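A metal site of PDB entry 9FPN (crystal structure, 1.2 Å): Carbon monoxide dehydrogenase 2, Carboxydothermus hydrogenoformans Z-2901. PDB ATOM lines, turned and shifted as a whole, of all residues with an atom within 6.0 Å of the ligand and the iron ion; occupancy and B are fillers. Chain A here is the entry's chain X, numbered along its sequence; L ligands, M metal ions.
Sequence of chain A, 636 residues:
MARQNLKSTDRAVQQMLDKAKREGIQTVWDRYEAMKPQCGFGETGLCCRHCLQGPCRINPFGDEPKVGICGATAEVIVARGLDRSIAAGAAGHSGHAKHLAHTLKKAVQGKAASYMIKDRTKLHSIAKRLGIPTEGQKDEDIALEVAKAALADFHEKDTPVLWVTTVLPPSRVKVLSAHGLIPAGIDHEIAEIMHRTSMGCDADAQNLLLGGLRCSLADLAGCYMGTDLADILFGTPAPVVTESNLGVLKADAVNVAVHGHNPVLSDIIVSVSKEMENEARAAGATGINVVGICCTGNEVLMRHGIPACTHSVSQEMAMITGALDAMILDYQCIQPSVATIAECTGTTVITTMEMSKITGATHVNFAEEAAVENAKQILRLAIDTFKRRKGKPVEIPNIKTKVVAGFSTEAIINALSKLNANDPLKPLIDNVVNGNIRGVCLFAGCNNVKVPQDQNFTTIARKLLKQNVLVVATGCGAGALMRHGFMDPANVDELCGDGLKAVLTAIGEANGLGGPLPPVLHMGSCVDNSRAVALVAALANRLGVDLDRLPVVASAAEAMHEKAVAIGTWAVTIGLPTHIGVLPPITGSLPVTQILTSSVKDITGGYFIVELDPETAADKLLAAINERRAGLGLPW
A sulfur (S2) of the ligand lies close to the side-chain hydroxyl (OG) of Ser 312 (3.7 Å).
SG of Cys 446 is bound to FE2 of the ligand (2.4 Å).
S4 of the ligand lies close to NZ of Lys 563, 3.4 Å away.
FE3 of the ligand is bound by SG of Cys 476 (2.3 Å).
FE1 of the ligand is bound by SG of Cys 333, at 2.3 Å.
The backbone NH of Cys 446 lies close to a sulfur (S1) of the ligand (3.3 Å).
A nickel atom (NI1) of the ligand is bound by the side-chain sulfur (SG) of Cys 526 (2.1 Å).
N of Cys 476 sits close to S1 of the ligand (3.5 Å).
The backbone carbonyl oxygen (O) of Gly 445 lies close to the backbone NH (N) of Cys 476, at 3.2 Å.
SG of Cys 295 sits close to ND2 of Asn 298.
The backbone NH (N) of Gly 477 is in hydrogen-bond range of the backbone carbonyl oxygen (O) of Gly 445.
ND1 of His 261 sits close to NZ of Lys 563 (3.4 Å).
The backbone NH (N) of Cys 295 is in hydrogen-bond range of the backbone carbonyl oxygen (O) of Gly 260.
SG of Cys 476 lies close to OG of Ser 312, 3.2 Å away.
The side-chain amino group (NZ) of Lys 563 sits at hydrogen-bond distance from the side-chain amide oxygen (OE1) of Gln 332 (2.7 Å).
N of Lys 563 sits at hydrogen-bond distance from ND1 of His 561 (2.9 Å).
A sulfur (S1) of the ligand sits close to the backbone carbonyl oxygen of Gly 445 (3.3 Å).
Residues that only touch the ligand: Met 560, His 561 and Cys 294.
Hydrophobic or aromatic side chains within 4 Å of the ligand: His 261, Met 560 and His 561.
The nearest printed residue that does not touch the ligand is Gly 475 (4.2 Å).
The iron ion is bound by a ring nitrogen (NE2) of His 261 (2.0 Å).
The iron ion is bound by S3 of the ligand.
The iron ion is bound by SG of Cys 295.
The iron ion is bound by SG of Cys 526 (2.5 Å).
The iron ion has four donor atoms within binding distance.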
ATOM      1  N   HIS A  93     -23.934  13.860  19.760  1.00  0.00           N
ATOM      2  CA  HIS A  93     -24.567  12.568  19.503  1.00  0.00           C
ATOM      3  C   HIS A  93     -24.527  12.239  18.030  1.00  0.00           C
ATOM      4  O   HIS A  93     -24.288  11.097  17.626  1.00  0.00           O
ATOM      5  CB  HIS A  93     -26.028  12.551  19.961  1.00  0.00           C
ATOM      6  CG  HIS A  93     -26.204  12.563  21.442  1.00  0.00           C
ATOM      7  ND1 HIS A  93     -27.060  13.431  22.046  1.00  0.00           N
ATOM      8  CD2 HIS A  93     -25.698  11.785  22.432  1.00  0.00           C
ATOM      9  CE1 HIS A  93     -27.058  13.218  23.349  1.00  0.00           C
ATOM     10  NE2 HIS A  93     -26.263  12.201  23.601  1.00  0.00           N
ATOM     11  N   GLY A 260     -15.337   7.236  27.172  1.00  0.00           N
ATOM     12  CA  GLY A 260     -15.847   8.083  26.115  1.00  0.00           C
ATOM     13  C   GLY A 260     -17.243   7.644  25.763  1.00  0.00           C
ATOM     14  O   GLY A 260     -18.012   7.281  26.668  1.00  0.00           O
ATOM     15  N   HIS A 261     -17.596   7.721  24.502  1.00  0.00           N
ATOM     16  CA  HIS A 261     -18.921   7.396  23.957  1.00  0.00           C
ATOM     17  C   HIS A 261     -18.925   6.495  22.731  1.00  0.00           C
ATOM     18  O   HIS A 261     -19.802   5.626  22.636  1.00  0.00           O
ATOM     19  CB  HIS A 261     -19.811   8.744  23.708  1.00  0.00           C
ATOM     20  CG  HIS A 261     -20.403   9.270  24.979  1.00  0.00           C
ATOM     21  ND1 HIS A 261     -19.631   9.851  25.955  1.00  0.00           N
ATOM     22  CD2 HIS A 261     -21.672   9.223  25.480  1.00  0.00           C
ATOM     23  CE1 HIS A 261     -20.375  10.066  27.030  1.00  0.00           C
ATOM     24  NE2 HIS A 261     -21.635   9.664  26.797  1.00  0.00           N
ATOM     25  N   CYS A 294     -18.018   5.570  31.881  1.00  0.00           N
ATOM     26  CA  CYS A 294     -18.990   6.314  31.092  1.00  0.00           C
ATOM     27  C   CYS A 294     -19.600   5.469  29.966  1.00  0.00           C
ATOM     28  O   CYS A 294     -19.793   4.264  30.135  1.00  0.00           O
ATOM     29  CB  CYS A 294     -18.379   7.652  30.645  1.00  0.00           C
ATOM     30  SG  CYS A 294     -18.156   8.842  32.008  1.00  0.00           S
ATOM     31  N   CYS A 295     -19.871   6.034  28.851  1.00  0.00           N
ATOM     32  CA  CYS A 295     -20.738   5.339  27.917  1.00  0.00           C
ATOM     33  C   CYS A 295     -20.008   4.373  27.003  1.00  0.00           C
ATOM     34  O   CYS A 295     -20.595   3.373  26.601  1.00  0.00           O
ATOM     35  CB  CYS A 295     -21.636   6.279  27.124  1.00  0.00           C
ATOM     36  SG  CYS A 295     -23.021   6.759  28.104  1.00  0.00           S
ATOM     37  N   ASN A 298     -20.590   1.668  29.028  1.00  0.00           N
ATOM     38  CA  ASN A 298     -21.945   1.151  28.860  1.00  0.00           C
ATOM     39  C   ASN A 298     -22.063   0.292  27.616  1.00  0.00           C
ATOM     40  O   ASN A 298     -22.728  -0.727  27.635  1.00  0.00           O
ATOM     41  CB  ASN A 298     -23.007   2.247  28.859  1.00  0.00           C
ATOM     42  CG  ASN A 298     -23.398   2.667  30.243  1.00  0.00           C
ATOM     43  OD1 ASN A 298     -23.610   1.870  31.127  1.00  0.00           O
ATOM     44  ND2 ASN A 298     -23.546   3.973  30.420  1.00  0.00           N
ATOM     45  N   SER A 312     -19.297   9.295  35.229  1.00  0.00           N
ATOM     46  CA  SER A 312     -18.880  10.657  35.005  1.00  0.00           C
ATOM     47  C   SER A 312     -18.113  11.354  36.111  1.00  0.00           C
ATOM     48  O   SER A 312     -16.882  11.502  36.008  1.00  0.00           O
ATOM     49  CB  SER A 312     -19.975  11.557  34.440  1.00  0.00           C
ATOM     50  OG  SER A 312     -21.040  11.703  35.356  1.00  0.00           O
ATOM     51  N   GLN A 332     -16.069  12.836  24.437  1.00  0.00           N
ATOM     52  CA  GLN A 332     -17.210  13.313  25.195  1.00  0.00           C
ATOM     53  C   GLN A 332     -17.158  12.836  26.642  1.00  0.00           C
ATOM     54  O   GLN A 332     -17.001  11.618  26.897  1.00  0.00           O
ATOM     55  CB  GLN A 332     -18.557  12.906  24.623  1.00  0.00           C
ATOM     56  CG  GLN A 332     -18.784  13.359  23.164  1.00  0.00           C
ATOM     57  CD  GLN A 332     -19.919  12.599  22.510  1.00  0.00           C
ATOM     58  OE1 GLN A 332     -20.767  11.955  23.176  1.00  0.00           O
ATOM     59  NE2 GLN A 332     -19.958  12.650  21.173  1.00  0.00           N
ATOM     60  N   CYS A 333     -17.287  13.778  27.580  1.00  0.00           N
ATOM     61  CA  CYS A 333     -17.500  13.515  29.013  1.00  0.00           C
ATOM     62  C   CYS A 333     -16.238  13.068  29.718  1.00  0.00           C
ATOM     63  O   CYS A 333     -16.295  12.643  30.866  1.00  0.00           O
ATOM     64  CB  CYS A 333     -18.674  12.530  29.188  1.00  0.00           C
ATOM     65  SG  CYS A 333     -20.165  13.189  28.465  1.00  0.00           S
ATOM     66  N   ALA A 444     -31.943   9.277  32.882  1.00  0.00           N
ATOM     67  CA  ALA A 444     -31.004   9.546  31.837  1.00  0.00           C
ATOM     68  C   ALA A 444     -30.033  10.608  32.320  1.00  0.00           C
ATOM     69  O   ALA A 444     -30.256  11.303  33.322  1.00  0.00           O
ATOM     70  CB  ALA A 444     -31.715  10.013  30.565  1.00  0.00           C
ATOM     71  N   GLY A 445     -28.954  10.726  31.570  1.00  0.00           N
ATOM     72  CA  GLY A 445     -28.009  11.788  31.771  1.00  0.00           C
ATOM     73  C   GLY A 445     -27.061  11.538  32.923  1.00  0.00           C
ATOM     74  O   GLY A 445     -26.891  10.437  33.449  1.00  0.00           O
ATOM     75  N   CYS A 446     -26.291  12.605  33.117  1.00  0.00           N
ATOM     76  CA  CYS A 446     -25.067  12.588  33.918  1.00  0.00           C
ATOM     77  C   CYS A 446     -25.148  12.735  35.428  1.00  0.00           C
ATOM     78  O   CYS A 446     -26.278  12.632  35.987  1.00  0.00           O
ATOM     79  CB  CYS A 446     -24.360  13.878  33.423  1.00  0.00           C
ATOM     80  SG  CYS A 446     -24.829  14.587  31.788  1.00  0.00           S
ATOM     81  N   ASN A 447     -23.985  12.608  36.094  1.00  0.00           N
ATOM     82  CA  ASN A 447     -23.798  13.170  37.415  1.00  0.00           C
ATOM     83  C   ASN A 447     -23.313  14.620  37.243  1.00  0.00           C
ATOM     84  O   ASN A 447     -22.842  15.004  36.165  1.00  0.00           O
ATOM     85  CB  ASN A 447     -22.748  12.416  38.232  1.00  0.00           C
ATOM     86  CG  ASN A 447     -23.077  10.935  38.573  1.00  0.00           C
ATOM     87  OD1 ASN A 447     -22.240  10.082  38.320  1.00  0.00           O
ATOM     88  ND2 ASN A 447     -24.222  10.690  39.187  1.00  0.00           N
ATOM     89  N   THR A 474     -30.358   4.846  31.411  1.00  0.00           N
ATOM     90  CA  THR A 474     -29.257   4.895  30.462  1.00  0.00           C
ATOM     91  C   THR A 474     -28.133   5.782  31.014  1.00  0.00           C
ATOM     92  O   THR A 474     -28.291   6.502  32.001  1.00  0.00           O
ATOM     93  CB  THR A 474     -29.688   5.505  29.133  1.00  0.00           C
ATOM     94  OG1 THR A 474     -30.062   6.862  29.391  1.00  0.00           O
ATOM     95  CG2 THR A 474     -30.859   4.747  28.509  1.00  0.00           C
ATOM     96  N   GLY A 475     -26.972   5.707  30.370  1.00  0.00           N
ATOM     97  CA  GLY A 475     -25.881   6.624  30.683  1.00  0.00           C
ATOM     98  C   GLY A 475     -25.490   6.569  32.149  1.00  0.00           C
ATOM     99  O   GLY A 475     -25.413   5.497  32.758  1.00  0.00           O
ATOM    100  N   CYS A 476     -25.240   7.748  32.727  1.00  0.00           N
ATOM    101  CA  CYS A 476     -24.832   7.841  34.122  1.00  0.00           C
ATOM    102  C   CYS A 476     -25.998   7.606  35.080  1.00  0.00           C
ATOM    103  O   CYS A 476     -25.773   7.273  36.250  1.00  0.00           O
ATOM    104  CB  CYS A 476     -24.176   9.192  34.410  1.00  0.00           C
ATOM    105  SG  CYS A 476     -22.561   9.395  33.652  1.00  0.00           S
ATOM    106  N   GLY A 477     -27.236   7.768  34.620  1.00  0.00           N
ATOM    107  CA  GLY A 477     -28.367   7.315  35.410  1.00  0.00           C
ATOM    108  C   GLY A 477     -28.305   5.824  35.650  1.00  0.00           C
ATOM    109  O   GLY A 477     -28.406   5.346  36.780  1.00  0.00           O
ATOM    110  N   SER A 525     -26.374   3.129  26.657  1.00  0.00           N
ATOM    111  CA  SER A 525     -25.624   4.360  26.621  1.00  0.00           C
ATOM    112  C   SER A 525     -26.518   5.552  26.385  1.00  0.00           C
ATOM    113  O   SER A 525     -27.743   5.465  26.259  1.00  0.00           O
ATOM    114  CB  SER A 525     -24.624   4.311  25.489  1.00  0.00           C
ATOM    115  OG  SER A 525     -25.381   4.214  24.268  1.00  0.00           O
ATOM    116  N   CYS A 526     -25.853   6.710  26.327  1.00  0.00           N
ATOM    117  CA  CYS A 526     -26.692   7.973  26.073  1.00  0.00           C
ATOM    118  C   CYS A 526     -27.444   8.019  24.654  1.00  0.00           C
ATOM    119  O   CYS A 526     -28.656   8.451  24.487  1.00  0.00           O
ATOM    120  CB  CYS A 526     -25.841   9.261  26.305  1.00  0.00           C
ATOM    121  SG  CYS A 526     -25.388   9.394  28.060  1.00  0.00           S
ATOM    122  N   MET A 560     -25.680  17.394  33.388  1.00  0.00           N
ATOM    123  CA  MET A 560     -24.450  18.149  33.227  1.00  0.00           C
ATOM    124  C   MET A 560     -24.207  18.578  31.769  1.00  0.00           C
ATOM    125  O   MET A 560     -24.014  19.764  31.481  1.00  0.00           O
ATOM    126  CB  MET A 560     -23.251  17.365  33.772  1.00  0.00           C
ATOM    127  CG  MET A 560     -21.930  18.075  33.682  1.00  0.00           C
ATOM    128  SD  MET A 560     -20.959  17.697  32.165  1.00  0.00           S
ATOM    129  CE  MET A 560     -20.743  15.943  32.267  1.00  0.00           C
ATOM    130  N   HIS A 561     -24.129  17.637  30.851  1.00  0.00           N
ATOM    131  CA  HIS A 561     -23.580  17.919  29.535  1.00  0.00           C
ATOM    132  C   HIS A 561     -24.617  18.590  28.613  1.00  0.00           C
ATOM    133  O   HIS A 561     -25.820  18.402  28.785  1.00  0.00           O
ATOM    134  CB  HIS A 561     -23.131  16.592  28.910  1.00  0.00           C
ATOM    135  CG  HIS A 561     -22.130  16.739  27.823  1.00  0.00           C
ATOM    136  ND1 HIS A 561     -22.483  17.065  26.502  1.00  0.00           N
ATOM    137  CD2 HIS A 561     -20.791  16.627  27.838  1.00  0.00           C
ATOM    138  CE1 HIS A 561     -21.381  17.158  25.776  1.00  0.00           C
ATOM    139  NE2 HIS A 561     -20.330  16.902  26.555  1.00  0.00           N
ATOM    140  N   LYS A 563     -25.221  17.545  25.845  1.00  0.00           N
ATOM    141  CA  LYS A 563     -25.979  16.403  25.349  1.00  0.00           C
ATOM    142  C   LYS A 563     -27.212  16.089  26.190  1.00  0.00           C
ATOM    143  O   LYS A 563     -28.249  15.663  25.643  1.00  0.00           O
ATOM    144  CB  LYS A 563     -25.075  15.183  25.326  1.00  0.00           C
ATOM    145  CG  LYS A 563     -24.098  15.136  24.149  1.00  0.00           C
ATOM    146  CD  LYS A 563     -23.194  13.907  24.191  1.00  0.00           C
ATOM    147  CE  LYS A 563     -22.188  13.931  25.280  1.00  0.00           C
ATOM    148  NZ  LYS A 563     -21.734  12.557  25.675  1.00  0.00           N
ATOM    149  N   ALA A 564     -27.108  16.230  27.502  1.00  0.00           N
ATOM    150  CA  ALA A 564     -28.242  15.978  28.382  1.00  0.00           C
ATOM    151  C   ALA A 564     -29.340  17.035  28.244  1.00  0.00           C
ATOM    152  O   ALA A 564     -30.545  16.708  28.300  1.00  0.00           O
ATOM    153  CB  ALA A 564     -27.750  15.838  29.823  1.00  0.00           C
ATOM    154  N   ILE A 567     -31.152  15.957  25.061  1.00  0.00           N
ATOM    155  CA  ILE A 567     -32.030  14.812  25.318  1.00  0.00           C
ATOM    156  C   ILE A 567     -33.256  15.270  26.080  1.00  0.00           C
ATOM    157  O   ILE A 567     -34.376  14.875  25.768  1.00  0.00           O
ATOM    158  CB  ILE A 567     -31.254  13.744  26.082  1.00  0.00           C
ATOM    159  CG1 ILE A 567     -30.227  13.039  25.189  1.00  0.00           C
ATOM    160  CG2 ILE A 567     -32.237  12.702  26.699  1.00  0.00           C
ATOM    161  CD1 ILE A 567     -29.118  12.319  25.936  1.00  0.00           C
HETATM  162 NI1  LIG L   1     -24.485  11.144  28.829  1.00  0.00          NI
HETATM  163 FE1  LIG L   1     -21.724  11.959  29.556  1.00  0.00          FE
HETATM  164 FE2  LIG L   1     -23.824  12.734  30.745  1.00  0.00          FE
HETATM  165 FE3  LIG L   1     -22.611  10.470  31.593  1.00  0.00          FE
HETATM  166  S1  LIG L   1     -24.768  10.659  30.928  1.00  0.00           S
HETATM  167  S2  LIG L   1     -21.745  12.587  31.817  1.00  0.00           S
HETATM  168  S3  LIG L   1     -21.354   9.695  29.878  1.00  0.00           S
HETATM  169  S4  LIG L   1     -23.583  13.044  28.538  1.00  0.00           S
HETATM  170 FE    FE M   1     -22.936   9.134  28.263  1.00  0.00          FE
